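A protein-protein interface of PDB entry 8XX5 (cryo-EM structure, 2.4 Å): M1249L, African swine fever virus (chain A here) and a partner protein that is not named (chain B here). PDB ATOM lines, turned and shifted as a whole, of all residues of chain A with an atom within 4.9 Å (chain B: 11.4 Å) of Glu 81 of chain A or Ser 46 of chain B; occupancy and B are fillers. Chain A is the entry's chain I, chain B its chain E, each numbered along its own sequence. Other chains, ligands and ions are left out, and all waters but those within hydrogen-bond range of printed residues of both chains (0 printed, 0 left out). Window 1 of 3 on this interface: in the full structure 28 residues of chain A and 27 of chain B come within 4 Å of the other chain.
No residue of chain B comes within 4 Å of Ala 80 of chain A. Printed residues of chain B within 4 Å of Glu 81 of chain A: Ser 45 and Ser 46. No residue of chain B comes within 4 Å of Gly 83 of chain A. Of the printed residues of chain A, Phe 41 of chain B touches Arg 78 and Ile 82. Of the printed residues of chain A, Ala 44 of chain B touches Arg 78 (3.1 Å). Printed residues of chain A within 4 Å of Ser 45 of chain B: Arg 78 (3.2 Å) and Glu 81 (3.6 Å). Ser 46 of chain B touches just one residue of chain A: Glu 81 (3.0 Å). The nearest residue of chain B that does not touch Glu 81 of chain A is Ala 44 of chain B (4.05 Å). The nearest printed residue of chain A that does not touch Ser 46 of chain B is Lys 164 of chain A (6.0 Å).
Among the printed residues, pairs that only touch across the chains: Glu 81 of chain A with Ser 45 of chain B (3.6 Å), Ile 82 of chain A with Phe 41 of chain B (3.8 Å) and Ile 82 of chain A with Gln 43 of chain B (3.8 Å).
O of Phe 41 of chain B lies within hydrogen-bond range of NH2 of Arg 78 of chain A (3.2 Å). The guanidinium group (NE) of Arg 78 of chain A lies within hydrogen-bond range of the side-chain hydroxyl (OG) of Ser 45 of chain B (3.2 Å). The side-chain carboxylate (OE1) of Glu 81 of chain A sits at hydrogen-bond distance from the backbone NH (N) of Ser 46 of chain B. The guanidinium group of Arg 78 of chain A lies close to the backbone NH of Ala 44 of chain B (3.1 Å).
Of the 19 printed residues of chain B, 5 touch a printed residue of chain A. Hydrophobic or aromatic side chains of chain B that line the printed part of chain A: Phe 41. Printed residues of chain A that touch a printed residue of chain B: Arg 78, Glu 81 and Ile 82. Hydrophobic or aromatic side chains of chain A that line the printed part of chain B: Ile 82. Among the printed residues, 7 pairs touch across the chains. Among the printed residues, no Asp or Glu carboxylate lies within 4 Å of a Lys or Arg side-chain nitrogen of the other chain.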
ATOM      1  N   MET A  77       3.819  -6.824 -14.778  1.00  0.00           N
ATOM      2  CA  MET A  77       2.777  -6.734 -13.761  1.00  0.00           C
ATOM      3  C   MET A  77       2.024  -8.049 -13.621  1.00  0.00           C
ATOM      4  O   MET A  77       1.720  -8.480 -12.504  1.00  0.00           O
ATOM      5  CB  MET A  77       1.821  -5.593 -14.096  1.00  0.00           C
ATOM      6  CG  MET A  77       2.253  -4.274 -13.502  1.00  0.00           C
ATOM      7  SD  MET A  77       2.715  -4.472 -11.773  1.00  0.00           S
ATOM      8  CE  MET A  77       1.344  -3.663 -10.968  1.00  0.00           C
ATOM      9  N   ARG A  78       1.716  -8.701 -14.744  1.00  0.00           N
ATOM     10  CA  ARG A  78       1.093 -10.019 -14.699  1.00  0.00           C
ATOM     11  C   ARG A  78       1.997 -11.024 -14.006  1.00  0.00           C
ATOM     12  O   ARG A  78       1.536 -11.840 -13.199  1.00  0.00           O
ATOM     13  CB  ARG A  78       0.766 -10.494 -16.115  1.00  0.00           C
ATOM     14  CG  ARG A  78      -0.475  -9.875 -16.721  1.00  0.00           C
ATOM     15  CD  ARG A  78      -1.002 -10.735 -17.855  1.00  0.00           C
ATOM     16  NE  ARG A  78      -1.515 -12.010 -17.368  1.00  0.00           N
ATOM     17  CZ  ARG A  78      -1.925 -13.000 -18.148  1.00  0.00           C
ATOM     18  NH1 ARG A  78      -1.907 -12.893 -19.467  1.00  0.00           N
ATOM     19  NH2 ARG A  78      -2.366 -14.126 -17.593  1.00  0.00           N
ATOM     20  N   MET A  79       3.293 -10.979 -14.315  1.00  0.00           N
ATOM     21  CA  MET A  79       4.241 -11.892 -13.686  1.00  0.00           C
ATOM     22  C   MET A  79       4.325 -11.666 -12.182  1.00  0.00           C
ATOM     23  O   MET A  79       4.401 -12.627 -11.406  1.00  0.00           O
ATOM     24  CB  MET A  79       5.606 -11.728 -14.345  1.00  0.00           C
ATOM     25  CG  MET A  79       6.618 -12.778 -13.983  1.00  0.00           C
ATOM     26  SD  MET A  79       7.656 -13.169 -15.394  1.00  0.00           S
ATOM     27  CE  MET A  79       7.459 -11.661 -16.322  1.00  0.00           C
ATOM     28  N   ALA A  80       4.315 -10.405 -11.751  1.00  0.00           N
ATOM     29  CA  ALA A  80       4.332 -10.113 -10.323  1.00  0.00           C
ATOM     30  C   ALA A  80       3.027 -10.532  -9.655  1.00  0.00           C
ATOM     31  O   ALA A  80       3.027 -10.966  -8.498  1.00  0.00           O
ATOM     32  CB  ALA A  80       4.604  -8.626 -10.098  1.00  0.00           C
ATOM     33  N   GLU A  81       1.905 -10.402 -10.367  1.00  0.00           N
ATOM     34  CA  GLU A  81       0.627 -10.860  -9.833  1.00  0.00           C
ATOM     35  C   GLU A  81       0.620 -12.372  -9.644  1.00  0.00           C
ATOM     36  O   GLU A  81       0.092 -12.877  -8.646  1.00  0.00           O
ATOM     37  CB  GLU A  81      -0.512 -10.423 -10.753  1.00  0.00           C
ATOM     38  CG  GLU A  81      -1.848 -11.074 -10.443  1.00  0.00           C
ATOM     39  CD  GLU A  81      -2.745 -11.169 -11.660  1.00  0.00           C
ATOM     40  OE1 GLU A  81      -3.386 -10.156 -12.006  1.00  0.00           O
ATOM     41  OE2 GLU A  81      -2.806 -12.257 -12.271  1.00  0.00           O
ATOM     42  N   ILE A  82       1.193 -13.111 -10.596  1.00  0.00           N
ATOM     43  CA  ILE A  82       1.354 -14.550 -10.414  1.00  0.00           C
ATOM     44  C   ILE A  82       2.235 -14.827  -9.202  1.00  0.00           C
ATOM     45  O   ILE A  82       1.940 -15.710  -8.387  1.00  0.00           O
ATOM     46  CB  ILE A  82       1.917 -15.192 -11.695  1.00  0.00           C
ATOM     47  CG1 ILE A  82       0.942 -14.996 -12.857  1.00  0.00           C
ATOM     48  CG2 ILE A  82       2.190 -16.669 -11.479  1.00  0.00           C
ATOM     49  CD1 ILE A  82       1.594 -15.020 -14.219  1.00  0.00           C
ATOM     50  N   GLY A  83       3.331 -14.081  -9.068  1.00  0.00           N
ATOM     51  CA  GLY A  83       4.078 -14.014  -7.832  1.00  0.00           C
ATOM     52  C   GLY A  83       4.992 -15.180  -7.535  1.00  0.00           C
ATOM     53  O   GLY A  83       5.589 -15.210  -6.451  1.00  0.00           O
ATOM     54  N   VAL A 161       3.166  -3.919  -7.418  1.00  0.00           N
ATOM     55  CA  VAL A 161       1.901  -4.540  -7.031  1.00  0.00           C
ATOM     56  C   VAL A 161       1.215  -3.721  -5.946  1.00  0.00           C
ATOM     57  O   VAL A 161      -0.003  -3.510  -5.985  1.00  0.00           O
ATOM     58  CB  VAL A 161       2.126  -5.998  -6.589  1.00  0.00           C
ATOM     59  CG1 VAL A 161       0.861  -6.570  -5.973  1.00  0.00           C
ATOM     60  CG2 VAL A 161       2.555  -6.845  -7.766  1.00  0.00           C
ATOM     61  N   LYS A 164      -0.299  -0.611  -7.504  1.00  0.00           N
ATOM     62  CA  LYS A 164      -1.513  -0.943  -8.244  1.00  0.00           C
ATOM     63  C   LYS A 164      -2.680  -1.203  -7.301  1.00  0.00           C
ATOM     64  O   LYS A 164      -3.799  -0.733  -7.536  1.00  0.00           O
ATOM     65  CB  LYS A 164      -1.264  -2.157  -9.137  1.00  0.00           C
ATOM     66  CG  LYS A 164      -2.317  -2.368 -10.211  1.00  0.00           C
ATOM     67  CD  LYS A 164      -2.277  -3.789 -10.754  1.00  0.00           C
ATOM     68  CE  LYS A 164      -2.232  -4.814  -9.632  1.00  0.00           C
ATOM     69  NZ  LYS A 164      -3.204  -5.922  -9.850  1.00  0.00           N
ATOM     70  N   GLY B  40       2.550 -19.050 -22.760  1.00  0.00           N
ATOM     71  CA  GLY B  40       2.383 -19.108 -21.325  1.00  0.00           C
ATOM     72  C   GLY B  40       1.330 -18.127 -20.860  1.00  0.00           C
ATOM     73  O   GLY B  40       0.453 -17.703 -21.619  1.00  0.00           O
ATOM     74  N   PHE B  41       1.434 -17.752 -19.587  1.00  0.00           N
ATOM     75  CA  PHE B  41       0.474 -16.864 -18.936  1.00  0.00           C
ATOM     76  C   PHE B  41      -0.953 -17.379 -19.117  1.00  0.00           C
ATOM     77  O   PHE B  41      -1.874 -16.644 -19.478  1.00  0.00           O
ATOM     78  CB  PHE B  41       0.607 -15.427 -19.445  1.00  0.00           C
ATOM     79  CG  PHE B  41       1.819 -14.709 -18.929  1.00  0.00           C
ATOM     80  CD1 PHE B  41       2.573 -15.246 -17.900  1.00  0.00           C
ATOM     81  CD2 PHE B  41       2.190 -13.486 -19.456  1.00  0.00           C
ATOM     82  CE1 PHE B  41       3.686 -14.584 -17.422  1.00  0.00           C
ATOM     83  CE2 PHE B  41       3.298 -12.821 -18.978  1.00  0.00           C
ATOM     84  CZ  PHE B  41       4.046 -13.370 -17.961  1.00  0.00           C
ATOM     85  N   VAL B  42      -1.118 -18.679 -18.861  1.00  0.00           N
ATOM     86  CA  VAL B  42      -2.446 -19.284 -18.872  1.00  0.00           C
ATOM     87  C   VAL B  42      -3.261 -18.898 -17.646  1.00  0.00           C
ATOM     88  O   VAL B  42      -4.472 -19.165 -17.611  1.00  0.00           O
ATOM     89  CB  VAL B  42      -2.351 -20.821 -18.964  1.00  0.00           C
ATOM     90  CG1 VAL B  42      -1.127 -21.230 -19.766  1.00  0.00           C
ATOM     91  CG2 VAL B  42      -2.315 -21.440 -17.581  1.00  0.00           C
ATOM     92  N   GLN B  43      -2.640 -18.258 -16.653  1.00  0.00           N
ATOM     93  CA  GLN B  43      -3.300 -18.023 -15.374  1.00  0.00           C
ATOM     94  C   GLN B  43      -4.496 -17.087 -15.509  1.00  0.00           C
ATOM     95  O   GLN B  43      -5.454 -17.202 -14.733  1.00  0.00           O
ATOM     96  CB  GLN B  43      -2.290 -17.462 -14.370  1.00  0.00           C
ATOM     97  CG  GLN B  43      -2.891 -17.009 -13.052  1.00  0.00           C
ATOM     98  CD  GLN B  43      -2.059 -17.424 -11.861  1.00  0.00           C
ATOM     99  OE1 GLN B  43      -1.180 -18.276 -11.969  1.00  0.00           O
ATOM    100  NE2 GLN B  43      -2.336 -16.823 -10.711  1.00  0.00           N
ATOM    101  N   ALA B  44      -4.456 -16.168 -16.478  1.00  0.00           N
ATOM    102  CA  ALA B  44      -5.478 -15.145 -16.688  1.00  0.00           C
ATOM    103  C   ALA B  44      -5.420 -14.106 -15.576  1.00  0.00           C
ATOM    104  O   ALA B  44      -5.464 -14.449 -14.391  1.00  0.00           O
ATOM    105  CB  ALA B  44      -6.882 -15.751 -16.795  1.00  0.00           C
ATOM    106  N   SER B  45      -5.316 -12.834 -15.957  1.00  0.00           N
ATOM    107  CA  SER B  45      -5.135 -11.763 -14.987  1.00  0.00           C
ATOM    108  C   SER B  45      -6.305 -11.700 -14.015  1.00  0.00           C
ATOM    109  O   SER B  45      -7.457 -11.968 -14.370  1.00  0.00           O
ATOM    110  CB  SER B  45      -4.979 -10.421 -15.701  1.00  0.00           C
ATOM    111  OG  SER B  45      -3.613 -10.104 -15.901  1.00  0.00           O
ATOM    112  N   SER B  46      -5.995 -11.346 -12.772  1.00  0.00           N
ATOM    113  CA  SER B  46      -7.019 -11.226 -11.746  1.00  0.00           C
ATOM    114  C   SER B  46      -7.982 -10.097 -12.084  1.00  0.00           C
ATOM    115  O   SER B  46      -7.634  -9.133 -12.771  1.00  0.00           O
ATOM    116  CB  SER B  46      -6.380 -10.978 -10.381  1.00  0.00           C
ATOM    117  OG  SER B  46      -5.777 -12.157  -9.881  1.00  0.00           O
ATOM    118  N   GLN B  47      -9.209 -10.227 -11.598  1.00  0.00           N
ATOM    119  CA  GLN B  47     -10.258  -9.254 -11.848  1.00  0.00           C
ATOM    120  C   GLN B  47     -10.527  -8.437 -10.594  1.00  0.00           C
ATOM    121  O   GLN B  47     -10.324  -8.904  -9.470  1.00  0.00           O
ATOM    122  CB  GLN B  47     -11.550  -9.940 -12.298  1.00  0.00           C
ATOM    123  CG  GLN B  47     -11.577 -10.319 -13.761  1.00  0.00           C
ATOM    124  CD  GLN B  47     -12.385 -11.572 -14.010  1.00  0.00           C
ATOM    125  OE1 GLN B  47     -12.859 -12.213 -13.075  1.00  0.00           O
ATOM    126  NE2 GLN B  47     -12.539 -11.934 -15.276  1.00  0.00           N
ATOM    127  N   THR B  48     -10.977  -7.205 -10.798  1.00  0.00           N
ATOM    128  CA  THR B  48     -11.473  -6.367  -9.720  1.00  0.00           C
ATOM    129  C   THR B  48     -12.991  -6.296  -9.813  1.00  0.00           C
ATOM    130  O   THR B  48     -13.559  -6.279 -10.911  1.00  0.00           O
ATOM    131  CB  THR B  48     -10.841  -4.967  -9.760  1.00  0.00           C
ATOM    132  OG1 THR B  48     -10.880  -4.385  -8.451  1.00  0.00           O
ATOM    133  CG2 THR B  48     -11.546  -4.047 -10.750  1.00  0.00           C
ATOM    134  N   LEU B  49     -13.649  -6.305  -8.659  1.00  0.00           N
ATOM    135  CA  LEU B  49     -15.105  -6.355  -8.595  1.00  0.00           C
ATOM    136  C   LEU B  49     -15.651  -4.935  -8.657  1.00  0.00           C
ATOM    137  O   LEU B  49     -15.578  -4.190  -7.676  1.00  0.00           O
ATOM    138  CB  LEU B  49     -15.563  -7.066  -7.326  1.00  0.00           C
ATOM    139  CG  LEU B  49     -16.975  -7.648  -7.352  1.00  0.00           C
ATOM    140  CD1 LEU B  49     -17.098  -8.714  -8.425  1.00  0.00           C
ATOM    141  CD2 LEU B  49     -17.340  -8.211  -5.994  1.00  0.00           C
ATOM    142  N   VAL B  50     -16.198  -4.561  -9.812  1.00  0.00           N
ATOM    143  CA  VAL B  50     -16.816  -3.254  -9.995  1.00  0.00           C
ATOM    144  C   VAL B  50     -18.302  -3.420  -9.695  1.00  0.00           C
ATOM    145  O   VAL B  50     -19.077  -3.855 -10.546  1.00  0.00           O
ATOM    146  CB  VAL B  50     -16.576  -2.702 -11.400  1.00  0.00           C
ATOM    147  CG1 VAL B  50     -17.304  -1.381 -11.581  1.00  0.00           C
ATOM    148  CG2 VAL B  50     -15.092  -2.529 -11.648  1.00  0.00           C
ATOM    149  N   VAL B 117     -17.963  -9.087 -17.836  1.00  0.00           N
ATOM    150  CA  VAL B 117     -16.538  -9.177 -17.539  1.00  0.00           C
ATOM    151  C   VAL B 117     -15.796  -8.435 -18.641  1.00  0.00           C
ATOM    152  O   VAL B 117     -15.843  -8.837 -19.810  1.00  0.00           O
ATOM    153  CB  VAL B 117     -16.069 -10.635 -17.436  1.00  0.00           C
ATOM    154  CG1 VAL B 117     -14.558 -10.712 -17.545  1.00  0.00           C
ATOM    155  CG2 VAL B 117     -16.547 -11.255 -16.135  1.00  0.00           C
ATOM    156  N   THR B 118     -15.122  -7.350 -18.276  1.00  0.00           N
ATOM    157  CA  THR B 118     -14.446  -6.515 -19.255  1.00  0.00           C
ATOM    158  C   THR B 118     -13.081  -7.094 -19.620  1.00  0.00           C
ATOM    159  O   THR B 118     -12.464  -7.803 -18.821  1.00  0.00           O
ATOM    160  CB  THR B 118     -14.270  -5.099 -18.716  1.00  0.00           C
ATOM    161  OG1 THR B 118     -13.107  -5.046 -17.880  1.00  0.00           O
ATOM    162  CG2 THR B 118     -15.481  -4.687 -17.911  1.00  0.00           C
ATOM    163  N   PRO B 119     -12.592  -6.813 -20.832  1.00  0.00           N
ATOM    164  CA  PRO B 119     -11.238  -7.264 -21.194  1.00  0.00           C
ATOM    165  C   PRO B 119     -10.154  -6.686 -20.303  1.00  0.00           C
ATOM    166  O   PRO B 119      -9.147  -7.358 -20.053  1.00  0.00           O
ATOM    167  CB  PRO B 119     -11.084  -6.795 -22.648  1.00  0.00           C
ATOM    168  CG  PRO B 119     -12.124  -5.744 -22.839  1.00  0.00           C
ATOM    169  CD  PRO B 119     -13.261  -6.114 -21.943  1.00  0.00           C
ATOM    170  N   GLU B 120     -10.329  -5.458 -19.814  1.00  0.00           N
ATOM    171  CA  GLU B 120      -9.328  -4.834 -18.959  1.00  0.00           C
ATOM    172  C   GLU B 120      -9.196  -5.518 -17.603  1.00  0.00           C
ATOM    173  O   GLU B 120      -8.222  -5.252 -16.890  1.00  0.00           O
ATOM    174  CB  GLU B 120      -9.654  -3.352 -18.767  1.00  0.00           C
ATOM    175  CG  GLU B 120     -10.465  -3.047 -17.521  1.00  0.00           C
ATOM    176  CD  GLU B 120     -11.225  -1.742 -17.630  1.00  0.00           C
ATOM    177  OE1 GLU B 120     -12.098  -1.633 -18.517  1.00  0.00           O
ATOM    178  OE2 GLU B 120     -10.954  -0.827 -16.825  1.00  0.00           O
ATOM    179  N   GLY B 121     -10.134  -6.384 -17.232  1.00  0.00           N
ATOM    180  CA  GLY B 121     -10.028  -7.124 -15.992  1.00  0.00           C
ATOM    181  C   GLY B 121     -10.975  -6.648 -14.912  1.00  0.00           C
ATOM    182  O   GLY B 121     -10.622  -6.633 -13.729  1.00  0.00           O
ATOM    183  N   GLN B 122     -12.183  -6.253 -15.304  1.00  0.00           N
ATOM    184  CA  GLN B 122     -13.208  -5.812 -14.372  1.00  0.00           C
ATOM    185  C   GLN B 122     -14.393  -6.760 -14.455  1.00  0.00           C
ATOM    186  O   GLN B 122     -14.861  -7.080 -15.551  1.00  0.00           O
ATOM    187  CB  GLN B 122     -13.665  -4.383 -14.673  1.00  0.00           C
ATOM    188  CG  GLN B 122     -12.693  -3.306 -14.239  1.00  0.00           C
ATOM    189  CD  GLN B 122     -13.115  -1.931 -14.711  1.00  0.00           C
ATOM    190  OE1 GLN B 122     -13.589  -1.766 -15.834  1.00  0.00           O
ATOM    191  NE2 GLN B 122     -12.945  -0.933 -13.852  1.00  0.00           N
ATOM    192  N   LYS B 123     -14.870  -7.208 -13.299  1.00  0.00           N
ATOM    193  CA  LYS B 123     -16.071  -8.034 -13.212  1.00  0.00           C
ATOM    194  C   LYS B 123     -17.201  -7.125 -12.745  1.00  0.00           C
ATOM    195  O   LYS B 123     -17.455  -6.979 -11.550  1.00  0.00           O
ATOM    196  CB  LYS B 123     -15.857  -9.214 -12.274  1.00  0.00           C
ATOM    197  CG  LYS B 123     -16.771 -10.392 -12.541  1.00  0.00           C
ATOM    198  CD  LYS B 123     -16.907 -11.268 -11.313  1.00  0.00           C
ATOM    199  CE  LYS B 123     -17.795 -12.465 -11.586  1.00  0.00           C
ATOM    200  NZ  LYS B 123     -17.509 -13.073 -12.911  1.00  0.00           N
ATOM    201  N   ILE B 124     -17.878  -6.500 -13.704  1.00  0.00           N
ATOM    202  CA  ILE B 124     -18.968  -5.580 -13.399  1.00  0.00           C
ATOM    203  C   ILE B 124     -20.175  -6.391 -12.947  1.00  0.00           C
ATOM    204  O   ILE B 124     -20.683  -7.236 -13.690  1.00  0.00           O
ATOM    205  CB  ILE B 124     -19.309  -4.705 -14.611  1.00  0.00           C
ATOM    206  CG1 ILE B 124     -18.141  -3.776 -14.937  1.00  0.00           C
ATOM    207  CG2 ILE B 124     -20.560  -3.901 -14.348  1.00  0.00           C
ATOM    208  CD1 ILE B 124     -18.245  -3.128 -16.290  1.00  0.00           C
